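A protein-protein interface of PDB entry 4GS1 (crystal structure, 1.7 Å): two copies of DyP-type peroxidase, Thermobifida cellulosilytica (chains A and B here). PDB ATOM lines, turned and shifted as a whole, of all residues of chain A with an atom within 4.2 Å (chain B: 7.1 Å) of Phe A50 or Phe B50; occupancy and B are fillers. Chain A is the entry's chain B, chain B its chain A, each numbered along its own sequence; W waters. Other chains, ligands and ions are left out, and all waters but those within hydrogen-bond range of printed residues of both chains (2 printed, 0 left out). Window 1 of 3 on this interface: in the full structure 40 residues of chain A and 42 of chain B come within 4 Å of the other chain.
Water W1 lies within hydrogen-bond range of the side-chain hydroxyl (OG1) of Thr B188 and the backbone carbonyl oxygen (O) of Glu A156. Water W2 lies within hydrogen-bond range of the side-chain hydroxyl of Thr A188 and the backbone carbonyl oxygen of Glu B156.
The side-chain carboxylate of Asp B157 sits at hydrogen-bond distance from the backbone NH of Met B159, 2.8 Å away. N of Phe B50 sits at hydrogen-bond distance from O of Ala B155 (3.0 Å). O of Ala A155 is in hydrogen-bond range of N of Phe A50, at 3.0 Å. O of Ala B49 sits at hydrogen-bond distance from N of Arg B186 (2.8 Å).
The backbone NH (N) of Thr A188 sits at hydrogen-bond distance from the side-chain carboxylate (OD1) of Asp B157, at 2.7 Å. N of Thr B188 sits at hydrogen-bond distance from OD1 of Asp A157, at 2.7 Å.
Printed residues of chain A that touch a printed residue of chain B: Phe A50, Asp A157, Pro A158, Phe A185 and Thr A188. Hydrophobic or aromatic side chains of chain B that line the printed part of chain A: Phe B50, Pro B158, Met B159 and Phe B185. Among the printed residues, 12 pairs touch across the chains.
Phe A50 touches just these residues of chain B: Phe B50 (3.3 Å) and Pro B158 (3.7 Å). Of the printed residues of chain B, Phe A185 touches Pro B158, Met B159 and Arg B183. Tyr A322 touches none of the printed residues of chain B. Of chain A, only Phe A50 and Pro A158 come within 4 Å of Phe B50. Ala B155 touches none of the printed residues of chain A. Of the printed residues of chain A, Arg B183 touches Phe A185. Printed residues of chain A within 4 Å of Arg B187: Asp A157. The nearest residue of chain B that does not touch Phe A50 is Thr B188 (5.1 Å). The nearest printed residue of chain A that does not touch Phe B50 is Thr A188 (5.2 Å). The nearest printed residue of chain A that does not touch Arg B187 is Pro A158 (5.1 Å).
Phe B50 touches its own counterpart, Phe A50. Phe A50 touches Pro B158, and with the chains exchanged Pro A158 touches Phe B50. Pro A158 touches Phe B185, and with the chains exchanged Phe A185 touches Pro B158. Pro A158 touches Thr B188, but with the chains exchanged Thr A188 does not touch Pro B158 (4.005 Å). Positions printed for both chains: 48, 49, 50, 51, 154, 155, 156, 157, 158, 161, 184, 185, 188 and 322.
Among the printed residues, merely in contact across the chains: Phe A50 with Phe B50 (3.3 Å), Phe A50 with Pro B158 (3.7 Å), Asp A157 with Arg B187 (3.6 Å), Pro A158 with Phe B50 (3.8 Å), Pro A158 with Phe B185 (3.7 Å), Pro A158 with Arg B186 (3.7 Å), Pro A158 with Thr B188 (3.96 Å), Phe A185 with Pro B158 (3.7 Å), Phe A185 with Met B159 (3.9 Å) and Phe A185 with Arg B183 (3.8 Å).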
ATOM      1  N   PRO A  48      -4.710 -36.754 -32.974  1.00  0.00           N
ATOM      2  CA  PRO A  48      -5.005 -35.593 -32.124  1.00  0.00           C
ATOM      3  C   PRO A  48      -6.475 -35.556 -31.732  1.00  0.00           C
ATOM      4  O   PRO A  48      -7.302 -36.204 -32.378  1.00  0.00           O
ATOM      5  CB  PRO A  48      -4.686 -34.397 -33.032  1.00  0.00           C
ATOM      6  CG  PRO A  48      -3.742 -34.938 -34.074  1.00  0.00           C
ATOM      7  CD  PRO A  48      -4.177 -36.361 -34.291  1.00  0.00           C
ATOM      8  N   ALA A  49      -6.805 -34.794 -30.692  1.00  0.00           N
ATOM      9  CA  ALA A  49      -8.167 -34.796 -30.164  1.00  0.00           C
ATOM     10  C   ALA A  49      -9.193 -34.107 -31.064  1.00  0.00           C
ATOM     11  O   ALA A  49     -10.389 -34.360 -30.927  1.00  0.00           O
ATOM     12  CB  ALA A  49      -8.198 -34.181 -28.754  1.00  0.00           C
ATOM     13  N   PHE A  50      -8.742 -33.234 -31.963  1.00  0.00           N
ATOM     14  CA  PHE A  50      -9.675 -32.473 -32.813  1.00  0.00           C
ATOM     15  C   PHE A  50      -9.372 -32.639 -34.287  1.00  0.00           C
ATOM     16  O   PHE A  50      -8.209 -32.798 -34.675  1.00  0.00           O
ATOM     17  CB  PHE A  50      -9.647 -30.982 -32.431  1.00  0.00           C
ATOM     18  CG  PHE A  50      -9.986 -30.745 -30.992  1.00  0.00           C
ATOM     19  CD1 PHE A  50     -11.308 -30.632 -30.590  1.00  0.00           C
ATOM     20  CD2 PHE A  50      -8.984 -30.687 -30.028  1.00  0.00           C
ATOM     21  CE1 PHE A  50     -11.627 -30.453 -29.251  1.00  0.00           C
ATOM     22  CE2 PHE A  50      -9.298 -30.511 -28.684  1.00  0.00           C
ATOM     23  CZ  PHE A  50     -10.631 -30.394 -28.302  1.00  0.00           C
ATOM     24  N   VAL A  51     -10.422 -32.590 -35.110  1.00  0.00           N
ATOM     25  CA  VAL A  51     -10.270 -32.662 -36.564  1.00  0.00           C
ATOM     26  C   VAL A  51     -11.221 -31.688 -37.251  1.00  0.00           C
ATOM     27  O   VAL A  51     -12.273 -31.354 -36.716  1.00  0.00           O
ATOM     28  CB  VAL A  51     -10.529 -34.101 -37.106  1.00  0.00           C
ATOM     29  CG1 VAL A  51     -12.043 -34.412 -37.172  1.00  0.00           C
ATOM     30  CG2 VAL A  51      -9.892 -34.296 -38.485  1.00  0.00           C
ATOM     31  N   GLY A 154      -5.810 -31.614 -38.359  1.00  0.00           N
ATOM     32  CA  GLY A 154      -5.990 -32.125 -37.014  1.00  0.00           C
ATOM     33  C   GLY A 154      -5.061 -31.443 -36.030  1.00  0.00           C
ATOM     34  O   GLY A 154      -3.966 -31.040 -36.391  1.00  0.00           O
ATOM     35  N   ALA A 155      -5.501 -31.315 -34.786  1.00  0.00           N
ATOM     36  CA  ALA A 155      -4.649 -30.775 -33.731  1.00  0.00           C
ATOM     37  C   ALA A 155      -5.202 -31.149 -32.379  1.00  0.00           C
ATOM     38  O   ALA A 155      -6.369 -31.506 -32.267  1.00  0.00           O
ATOM     39  CB  ALA A 155      -4.533 -29.263 -33.856  1.00  0.00           C
ATOM     40  N   GLU A 156      -4.366 -31.065 -31.350  1.00  0.00           N
ATOM     41  CA  GLU A 156      -4.792 -31.399 -29.993  1.00  0.00           C
ATOM     42  C   GLU A 156      -5.482 -30.203 -29.330  1.00  0.00           C
ATOM     43  O   GLU A 156      -6.006 -30.318 -28.224  1.00  0.00           O
ATOM     44  CB  GLU A 156      -3.574 -31.854 -29.169  1.00  0.00           C
ATOM     45  CG  GLU A 156      -3.870 -32.407 -27.760  1.00  0.00           C
ATOM     46  CD  GLU A 156      -4.592 -33.750 -27.762  1.00  0.00           C
ATOM     47  OE1 GLU A 156      -4.643 -34.424 -28.814  1.00  0.00           O
ATOM     48  OE2 GLU A 156      -5.105 -34.144 -26.691  1.00  0.00           O
ATOM     49  N   ASP A 157      -5.499 -29.063 -30.019  1.00  0.00           N
ATOM     50  CA  ASP A 157      -6.115 -27.850 -29.476  1.00  0.00           C
ATOM     51  C   ASP A 157      -7.019 -27.197 -30.521  1.00  0.00           C
ATOM     52  O   ASP A 157      -6.628 -27.091 -31.682  1.00  0.00           O
ATOM     53  CB  ASP A 157      -5.032 -26.864 -29.027  1.00  0.00           C
ATOM     54  CG  ASP A 157      -5.615 -25.627 -28.401  1.00  0.00           C
ATOM     55  OD1 ASP A 157      -5.849 -25.636 -27.171  1.00  0.00           O
ATOM     56  OD2 ASP A 157      -5.869 -24.650 -29.140  1.00  0.00           O
ATOM     57  N   PRO A 158      -8.233 -26.767 -30.118  1.00  0.00           N
ATOM     58  CA  PRO A 158      -9.193 -26.256 -31.104  1.00  0.00           C
ATOM     59  C   PRO A 158      -8.826 -24.879 -31.673  1.00  0.00           C
ATOM     60  O   PRO A 158      -9.253 -24.556 -32.780  1.00  0.00           O
ATOM     61  CB  PRO A 158     -10.506 -26.175 -30.302  1.00  0.00           C
ATOM     62  CG  PRO A 158     -10.040 -25.929 -28.879  1.00  0.00           C
ATOM     63  CD  PRO A 158      -8.809 -26.804 -28.756  1.00  0.00           C
ATOM     64  N   LEU A 161      -6.133 -25.518 -34.231  1.00  0.00           N
ATOM     65  CA  LEU A 161      -6.838 -26.073 -35.384  1.00  0.00           C
ATOM     66  C   LEU A 161      -7.558 -25.008 -36.202  1.00  0.00           C
ATOM     67  O   LEU A 161      -7.409 -24.971 -37.419  1.00  0.00           O
ATOM     68  CB  LEU A 161      -7.828 -27.157 -34.943  1.00  0.00           C
ATOM     69  CG  LEU A 161      -8.708 -27.759 -36.040  1.00  0.00           C
ATOM     70  CD1 LEU A 161      -7.863 -28.386 -37.120  1.00  0.00           C
ATOM     71  CD2 LEU A 161      -9.663 -28.793 -35.432  1.00  0.00           C
ATOM     72  N   GLY A 184     -14.835 -32.412 -35.697  1.00  0.00           N
ATOM     73  CA  GLY A 184     -15.028 -33.540 -34.797  1.00  0.00           C
ATOM     74  C   GLY A 184     -14.059 -33.527 -33.630  1.00  0.00           C
ATOM     75  O   GLY A 184     -13.045 -32.826 -33.667  1.00  0.00           O
ATOM     76  N   PHE A 185     -14.372 -34.294 -32.587  1.00  0.00           N
ATOM     77  CA  PHE A 185     -13.518 -34.352 -31.405  1.00  0.00           C
ATOM     78  C   PHE A 185     -13.448 -35.750 -30.810  1.00  0.00           C
ATOM     79  O   PHE A 185     -14.321 -36.592 -31.047  1.00  0.00           O
ATOM     80  CB  PHE A 185     -14.036 -33.397 -30.321  1.00  0.00           C
ATOM     81  CG  PHE A 185     -15.432 -33.711 -29.850  1.00  0.00           C
ATOM     82  CD1 PHE A 185     -15.648 -34.557 -28.766  1.00  0.00           C
ATOM     83  CD2 PHE A 185     -16.532 -33.168 -30.496  1.00  0.00           C
ATOM     84  CE1 PHE A 185     -16.936 -34.852 -28.339  1.00  0.00           C
ATOM     85  CE2 PHE A 185     -17.826 -33.460 -30.073  1.00  0.00           C
ATOM     86  CZ  PHE A 185     -18.025 -34.304 -28.989  1.00  0.00           C
ATOM     87  N   THR A 188      -9.564 -35.283 -24.882  1.00  0.00           N
ATOM     88  CA  THR A 188      -8.177 -34.814 -24.904  1.00  0.00           C
ATOM     89  C   THR A 188      -7.284 -35.695 -24.046  1.00  0.00           C
ATOM     90  O   THR A 188      -7.729 -36.281 -23.050  1.00  0.00           O
ATOM     91  CB  THR A 188      -8.043 -33.357 -24.425  1.00  0.00           C
ATOM     92  OG1 THR A 188      -8.535 -33.247 -23.081  1.00  0.00           O
ATOM     93  CG2 THR A 188      -8.818 -32.408 -25.349  1.00  0.00           C
ATOM     94  N   TYR A 322     -14.113 -39.562 -35.513  1.00  0.00           N
ATOM     95  CA  TYR A 322     -14.257 -38.527 -34.498  1.00  0.00           C
ATOM     96  C   TYR A 322     -15.728 -38.369 -34.166  1.00  0.00           C
ATOM     97  O   TYR A 322     -16.594 -38.698 -34.984  1.00  0.00           O
ATOM     98  CB  TYR A 322     -13.677 -37.178 -34.995  1.00  0.00           C
ATOM     99  CG  TYR A 322     -12.160 -37.167 -34.962  1.00  0.00           C
ATOM    100  CD1 TYR A 322     -11.476 -36.518 -33.943  1.00  0.00           C
ATOM    101  CD2 TYR A 322     -11.421 -37.832 -35.932  1.00  0.00           C
ATOM    102  CE1 TYR A 322     -10.080 -36.531 -33.893  1.00  0.00           C
ATOM    103  CE2 TYR A 322     -10.022 -37.862 -35.883  1.00  0.00           C
ATOM    104  CZ  TYR A 322      -9.369 -37.205 -34.860  1.00  0.00           C
ATOM    105  OH  TYR A 322      -7.988 -37.232 -34.807  1.00  0.00           O
ATOM    106  N   ALA B  47     -12.287 -19.976 -16.273  1.00  0.00           N
ATOM    107  CA  ALA B  47     -13.249 -20.483 -17.252  1.00  0.00           C
ATOM    108  C   ALA B  47     -12.678 -21.692 -17.972  1.00  0.00           C
ATOM    109  O   ALA B  47     -11.542 -21.654 -18.449  1.00  0.00           O
ATOM    110  CB  ALA B  47     -13.615 -19.402 -18.256  1.00  0.00           C
ATOM    111  N   PRO B  48     -13.459 -22.776 -18.050  1.00  0.00           N
ATOM    112  CA  PRO B  48     -13.030 -23.960 -18.809  1.00  0.00           C
ATOM    113  C   PRO B  48     -12.912 -23.675 -20.302  1.00  0.00           C
ATOM    114  O   PRO B  48     -13.505 -22.710 -20.805  1.00  0.00           O
ATOM    115  CB  PRO B  48     -14.161 -24.959 -18.566  1.00  0.00           C
ATOM    116  CG  PRO B  48     -14.787 -24.508 -17.252  1.00  0.00           C
ATOM    117  CD  PRO B  48     -14.719 -23.008 -17.321  1.00  0.00           C
ATOM    118  N   ALA B  49     -12.179 -24.524 -21.017  1.00  0.00           N
ATOM    119  CA  ALA B  49     -11.921 -24.284 -22.440  1.00  0.00           C
ATOM    120  C   ALA B  49     -13.124 -24.473 -23.365  1.00  0.00           C
ATOM    121  O   ALA B  49     -13.103 -23.967 -24.487  1.00  0.00           O
ATOM    122  CB  ALA B  49     -10.748 -25.132 -22.920  1.00  0.00           C
ATOM    123  N   PHE B  50     -14.151 -25.205 -22.923  1.00  0.00           N
ATOM    124  CA  PHE B  50     -15.313 -25.498 -23.781  1.00  0.00           C
ATOM    125  C   PHE B  50     -16.615 -25.097 -23.121  1.00  0.00           C
ATOM    126  O   PHE B  50     -16.747 -25.170 -21.895  1.00  0.00           O
ATOM    127  CB  PHE B  50     -15.349 -26.983 -24.185  1.00  0.00           C
ATOM    128  CG  PHE B  50     -14.109 -27.416 -24.902  1.00  0.00           C
ATOM    129  CD1 PHE B  50     -14.004 -27.271 -26.275  1.00  0.00           C
ATOM    130  CD2 PHE B  50     -13.033 -27.917 -24.194  1.00  0.00           C
ATOM    131  CE1 PHE B  50     -12.836 -27.626 -26.930  1.00  0.00           C
ATOM    132  CE2 PHE B  50     -11.856 -28.271 -24.836  1.00  0.00           C
ATOM    133  CZ  PHE B  50     -11.764 -28.124 -26.213  1.00  0.00           C
ATOM    134  N   VAL B  51     -17.565 -24.657 -23.941  1.00  0.00           N
ATOM    135  CA  VAL B  51     -18.894 -24.315 -23.451  1.00  0.00           C
ATOM    136  C   VAL B  51     -19.956 -24.851 -24.394  1.00  0.00           C
ATOM    137  O   VAL B  51     -19.712 -25.019 -25.591  1.00  0.00           O
ATOM    138  CB  VAL B  51     -19.066 -22.783 -23.265  1.00  0.00           C
ATOM    139  CG1 VAL B  51     -19.285 -22.070 -24.607  1.00  0.00           C
ATOM    140  CG2 VAL B  51     -20.231 -22.491 -22.313  1.00  0.00           C
ATOM    141  N   HIS B  52     -21.127 -25.163 -23.854  1.00  0.00           N
ATOM    142  CA  HIS B  52     -22.291 -25.429 -24.692  1.00  0.00           C
ATOM    143  C   HIS B  52     -23.444 -24.684 -24.034  1.00  0.00           C
ATOM    144  O   HIS B  52     -23.802 -24.969 -22.888  1.00  0.00           O
ATOM    145  CB  HIS B  52     -22.573 -26.937 -24.791  1.00  0.00           C
ATOM    146  CG  HIS B  52     -23.433 -27.327 -25.956  1.00  0.00           C
ATOM    147  ND1 HIS B  52     -23.455 -28.614 -26.470  1.00  0.00           N
ATOM    148  CD2 HIS B  52     -24.324 -26.622 -26.694  1.00  0.00           C
ATOM    149  CE1 HIS B  52     -24.300 -28.672 -27.474  1.00  0.00           C
ATOM    150  NE2 HIS B  52     -24.852 -27.479 -27.635  1.00  0.00           N
ATOM    151  N   MET B 106     -18.919 -27.708 -15.029  1.00  0.00           N
ATOM    152  CA  MET B 106     -19.771 -26.753 -14.319  1.00  0.00           C
ATOM    153  C   MET B 106     -21.082 -26.514 -15.073  1.00  0.00           C
ATOM    154  O   MET B 106     -21.109 -26.485 -16.306  1.00  0.00           O
ATOM    155  CB  MET B 106     -19.031 -25.428 -14.087  1.00  0.00           C
ATOM    156  CG  MET B 106     -18.351 -24.874 -15.320  1.00  0.00           C
ATOM    157  SD  MET B 106     -17.593 -23.265 -15.024  1.00  0.00           S
ATOM    158  CE  MET B 106     -16.252 -23.708 -13.930  1.00  0.00           C
ATOM    159  N   VAL B 153     -23.308 -25.135 -19.967  1.00  0.00           N
ATOM    160  CA  VAL B 153     -22.504 -26.255 -19.480  1.00  0.00           C
ATOM    161  C   VAL B 153     -21.074 -26.043 -19.942  1.00  0.00           C
ATOM    162  O   VAL B 153     -20.827 -25.759 -21.120  1.00  0.00           O
ATOM    163  CB  VAL B 153     -23.030 -27.607 -20.023  1.00  0.00           C
ATOM    164  CG1 VAL B 153     -22.362 -28.754 -19.287  1.00  0.00           C
ATOM    165  CG2 VAL B 153     -24.544 -27.689 -19.862  1.00  0.00           C
ATOM    166  N   GLY B 154     -20.124 -26.144 -19.017  1.00  0.00           N
ATOM    167  CA  GLY B 154     -18.736 -25.939 -19.393  1.00  0.00           C
ATOM    168  C   GLY B 154     -17.822 -27.028 -18.865  1.00  0.00           C
ATOM    169  O   GLY B 154     -18.088 -27.623 -17.826  1.00  0.00           O
ATOM    170  N   ALA B 155     -16.750 -27.294 -19.602  1.00  0.00           N
ATOM    171  CA  ALA B 155     -15.733 -28.243 -19.154  1.00  0.00           C
ATOM    172  C   ALA B 155     -14.448 -28.030 -19.923  1.00  0.00           C
ATOM    173  O   ALA B 155     -14.446 -27.426 -20.988  1.00  0.00           O
ATOM    174  CB  ALA B 155     -16.219 -29.664 -19.315  1.00  0.00           C
ATOM    175  N   GLU B 156     -13.350 -28.552 -19.390  1.00  0.00           N
ATOM    176  CA  GLU B 156     -12.052 -28.405 -20.038  1.00  0.00           C
ATOM    177  C   GLU B 156     -11.847 -29.468 -21.129  1.00  0.00           C
ATOM    178  O   GLU B 156     -10.849 -29.458 -21.861  1.00  0.00           O
ATOM    179  CB  GLU B 156     -10.961 -28.476 -18.960  1.00  0.00           C
ATOM    180  CG  GLU B 156      -9.541 -28.186 -19.427  1.00  0.00           C
ATOM    181  CD  GLU B 156      -9.314 -26.748 -19.873  1.00  0.00           C
ATOM    182  OE1 GLU B 156     -10.125 -25.853 -19.534  1.00  0.00           O
ATOM    183  OE2 GLU B 156      -8.291 -26.499 -20.559  1.00  0.00           O
ATOM    184  N   ASP B 157     -12.805 -30.386 -21.247  1.00  0.00           N
ATOM    185  CA  ASP B 157     -12.714 -31.461 -22.228  1.00  0.00           C
ATOM    186  C   ASP B 157     -14.034 -31.595 -22.991  1.00  0.00           C
ATOM    187  O   ASP B 157     -15.104 -31.525 -22.382  1.00  0.00           O
ATOM    188  CB  ASP B 157     -12.402 -32.782 -21.524  1.00  0.00           C
ATOM    189  CG  ASP B 157     -12.257 -33.923 -22.496  1.00  0.00           C
ATOM    190  OD1 ASP B 157     -11.137 -34.112 -23.027  1.00  0.00           O
ATOM    191  OD2 ASP B 157     -13.265 -34.620 -22.752  1.00  0.00           O
ATOM    192  N   PRO B 158     -13.975 -31.789 -24.323  1.00  0.00           N
ATOM    193  CA  PRO B 158     -15.225 -31.834 -25.091  1.00  0.00           C
ATOM    194  C   PRO B 158     -16.059 -33.101 -24.909  1.00  0.00           C
ATOM    195  O   PRO B 158     -17.273 -33.051 -25.117  1.00  0.00           O
ATOM    196  CB  PRO B 158     -14.746 -31.718 -26.546  1.00  0.00           C
ATOM    197  CG  PRO B 158     -13.369 -32.339 -26.521  1.00  0.00           C
ATOM    198  CD  PRO B 158     -12.787 -31.897 -25.194  1.00  0.00           C
ATOM    199  N   MET B 159     -15.423 -34.212 -24.545  1.00  0.00           N
ATOM    200  CA  MET B 159     -16.146 -35.453 -24.292  1.00  0.00           C
ATOM    201  C   MET B 159     -16.870 -35.390 -22.946  1.00  0.00           C
ATOM    202  O   MET B 159     -18.027 -35.806 -22.831  1.00  0.00           O
ATOM    203  CB  MET B 159     -15.198 -36.658 -24.359  1.00  0.00           C
ATOM    204  CG  MET B 159     -15.899 -37.994 -24.514  1.00  0.00           C
ATOM    205  SD  MET B 159     -16.703 -38.113 -26.133  1.00  0.00           S
ATOM    206  CE  MET B 159     -17.384 -39.768 -26.051  1.00  0.00           C
ATOM    207  N   LEU B 161     -17.827 -32.617 -21.612  1.00  0.00           N
ATOM    208  CA  LEU B 161     -18.912 -31.673 -21.905  1.00  0.00           C
ATOM    209  C   LEU B 161     -20.098 -32.342 -22.611  1.00  0.00           C
ATOM    210  O   LEU B 161     -21.254 -32.165 -22.211  1.00  0.00           O
ATOM    211  CB  LEU B 161     -18.389 -30.511 -22.756  1.00  0.00           C
ATOM    212  CG  LEU B 161     -19.444 -29.477 -23.175  1.00  0.00           C
ATOM    213  CD1 LEU B 161     -20.089 -28.914 -21.933  1.00  0.00           C
ATOM    214  CD2 LEU B 161     -18.805 -28.355 -23.980  1.00  0.00           C
ATOM    215  N   ARG B 183     -22.169 -24.272 -29.365  1.00  0.00           N
ATOM    216  CA  ARG B 183     -20.948 -24.730 -28.718  1.00  0.00           C
ATOM    217  C   ARG B 183     -19.808 -23.747 -29.006  1.00  0.00           C
ATOM    218  O   ARG B 183     -19.704 -23.199 -30.105  1.00  0.00           O
ATOM    219  CB  ARG B 183     -20.559 -26.120 -29.251  1.00  0.00           C
ATOM    220  CG  ARG B 183     -21.584 -27.213 -28.954  1.00  0.00           C
ATOM    221  CD  ARG B 183     -21.234 -28.544 -29.640  1.00  0.00           C
ATOM    222  NE  ARG B 183     -20.030 -29.142 -29.066  1.00  0.00           N
ATOM    223  CZ  ARG B 183     -18.863 -29.242 -29.698  1.00  0.00           C
ATOM    224  NH1 ARG B 183     -18.738 -28.794 -30.938  1.00  0.00           N
ATOM    225  NH2 ARG B 183     -17.821 -29.788 -29.087  1.00  0.00           N
ATOM    226  N   GLY B 184     -18.946 -23.538 -28.020  1.00  0.00           N
ATOM    227  CA  GLY B 184     -17.798 -22.662 -28.194  1.00  0.00           C
ATOM    228  C   GLY B 184     -16.546 -23.175 -27.509  1.00  0.00           C
ATOM    229  O   GLY B 184     -16.603 -24.104 -26.699  1.00  0.00           O
ATOM    230  N   PHE B 185     -15.406 -22.576 -27.842  1.00  0.00           N
ATOM    231  CA  PHE B 185     -14.118 -23.026 -27.327  1.00  0.00           C
ATOM    232  C   PHE B 185     -13.167 -21.856 -27.112  1.00  0.00           C
ATOM    233  O   PHE B 185     -13.350 -20.768 -27.678  1.00  0.00           O
ATOM    234  CB  PHE B 185     -13.472 -24.028 -28.307  1.00  0.00           C
ATOM    235  CG  PHE B 185     -13.192 -23.444 -29.680  1.00  0.00           C
ATOM    236  CD1 PHE B 185     -11.982 -22.819 -29.954  1.00  0.00           C
ATOM    237  CD2 PHE B 185     -14.144 -23.525 -30.686  1.00  0.00           C
ATOM    238  CE1 PHE B 185     -11.729 -22.277 -31.219  1.00  0.00           C
ATOM    239  CE2 PHE B 185     -13.899 -22.984 -31.961  1.00  0.00           C
ATOM    240  CZ  PHE B 185     -12.685 -22.360 -32.214  1.00  0.00           C
ATOM    241  N   ARG B 186     -12.160 -22.105 -26.279  1.00  0.00           N
ATOM    242  CA  ARG B 186     -10.986 -21.249 -26.103  1.00  0.00           C
ATOM    243  C   ARG B 186      -9.792 -22.183 -26.188  1.00  0.00           C
ATOM    244  O   ARG B 186      -9.963 -23.404 -26.202  1.00  0.00           O
ATOM    245  CB  ARG B 186     -10.992 -20.599 -24.722  1.00  0.00           C
ATOM    246  CG  ARG B 186     -12.131 -19.620 -24.477  1.00  0.00           C
ATOM    247  CD  ARG B 186     -12.153 -19.211 -23.014  1.00  0.00           C
ATOM    248  NE  ARG B 186     -13.122 -18.152 -22.754  1.00  0.00           N
ATOM    249  CZ  ARG B 186     -13.083 -17.374 -21.683  1.00  0.00           C
ATOM    250  NH1 ARG B 186     -12.120 -17.549 -20.776  1.00  0.00           N
ATOM    251  NH2 ARG B 186     -13.994 -16.423 -21.518  1.00  0.00           N
ATOM    252  N   ARG B 187      -8.582 -21.640 -26.238  1.00  0.00           N
ATOM    253  CA  ARG B 187      -7.409 -22.511 -26.189  1.00  0.00           C
ATOM    254  C   ARG B 187      -7.422 -23.332 -24.903  1.00  0.00           C
ATOM    255  O   ARG B 187      -7.857 -22.853 -23.852  1.00  0.00           O
ATOM    256  CB  ARG B 187      -6.109 -21.700 -26.304  1.00  0.00           C
ATOM    257  CG  ARG B 187      -5.489 -21.240 -24.974  1.00  0.00           C
ATOM    258  CD  ARG B 187      -6.345 -20.210 -24.246  1.00  0.00           C
ATOM    259  NE  ARG B 187      -5.650 -19.647 -23.083  1.00  0.00           N
ATOM    260  CZ  ARG B 187      -5.618 -20.210 -21.877  1.00  0.00           C
ATOM    261  NH1 ARG B 187      -6.242 -21.360 -21.663  1.00  0.00           N
ATOM    262  NH2 ARG B 187      -4.960 -19.619 -20.883  1.00  0.00           N
ATOM    263  N   THR B 188      -6.968 -24.581 -24.979  1.00  0.00           N
ATOM    264  CA  THR B 188      -6.905 -25.411 -23.780  1.00  0.00           C
ATOM    265  C   THR B 188      -5.712 -25.031 -22.915  1.00  0.00           C
ATOM    266  O   THR B 188      -4.683 -24.581 -23.426  1.00  0.00           O
ATOM    267  CB  THR B 188      -6.821 -26.911 -24.121  1.00  0.00           C
ATOM    268  OG1 THR B 188      -5.642 -27.169 -24.901  1.00  0.00           O
ATOM    269  CG2 THR B 188      -8.053 -27.347 -24.910  1.00  0.00           C
ATOM    270  N   ARG B 320     -17.477 -12.987 -20.651  1.00  0.00           N
ATOM    271  CA  ARG B 320     -16.964 -14.357 -20.507  1.00  0.00           C
ATOM    272  C   ARG B 320     -17.376 -15.128 -21.755  1.00  0.00           C
ATOM    273  O   ARG B 320     -18.201 -16.039 -21.705  1.00  0.00           O
ATOM    274  CB  ARG B 320     -17.527 -15.010 -19.229  1.00  0.00           C
ATOM    275  CG  ARG B 320     -16.890 -16.343 -18.810  1.00  0.00           C
ATOM    276  CD  ARG B 320     -17.514 -16.823 -17.490  1.00  0.00           C
ATOM    277  NE  ARG B 320     -17.053 -18.144 -17.045  1.00  0.00           N
ATOM    278  CZ  ARG B 320     -17.531 -19.303 -17.495  1.00  0.00           C
ATOM    279  NH1 ARG B 320     -18.469 -19.322 -18.441  1.00  0.00           N
ATOM    280  NH2 ARG B 320     -17.057 -20.448 -17.009  1.00  0.00           N
ATOM    281  N   TYR B 322     -16.777 -17.037 -25.774  1.00  0.00           N
ATOM    282  CA  TYR B 322     -16.090 -18.186 -26.363  1.00  0.00           C
ATOM    283  C   TYR B 322     -16.074 -18.011 -27.871  1.00  0.00           C
ATOM    284  O   TYR B 322     -16.892 -17.274 -28.415  1.00  0.00           O
ATOM    285  CB  TYR B 322     -16.800 -19.498 -25.979  1.00  0.00           C
ATOM    286  CG  TYR B 322     -16.506 -19.926 -24.554  1.00  0.00           C
ATOM    287  CD1 TYR B 322     -15.576 -20.918 -24.287  1.00  0.00           C
ATOM    288  CD2 TYR B 322     -17.146 -19.320 -23.480  1.00  0.00           C
ATOM    289  CE1 TYR B 322     -15.282 -21.296 -22.987  1.00  0.00           C
ATOM    290  CE2 TYR B 322     -16.859 -19.688 -22.177  1.00  0.00           C
ATOM    291  CZ  TYR B 322     -15.929 -20.677 -21.940  1.00  0.00           C
ATOM    292  OH  TYR B 322     -15.639 -21.040 -20.643  1.00  0.00           O
HETATM  293  O   HOH W   1      -5.315 -29.980 -25.418  1.00  0.00           O
HETATM  294  O   HOH W   2      -8.159 -30.589 -21.940  1.00  0.00           O
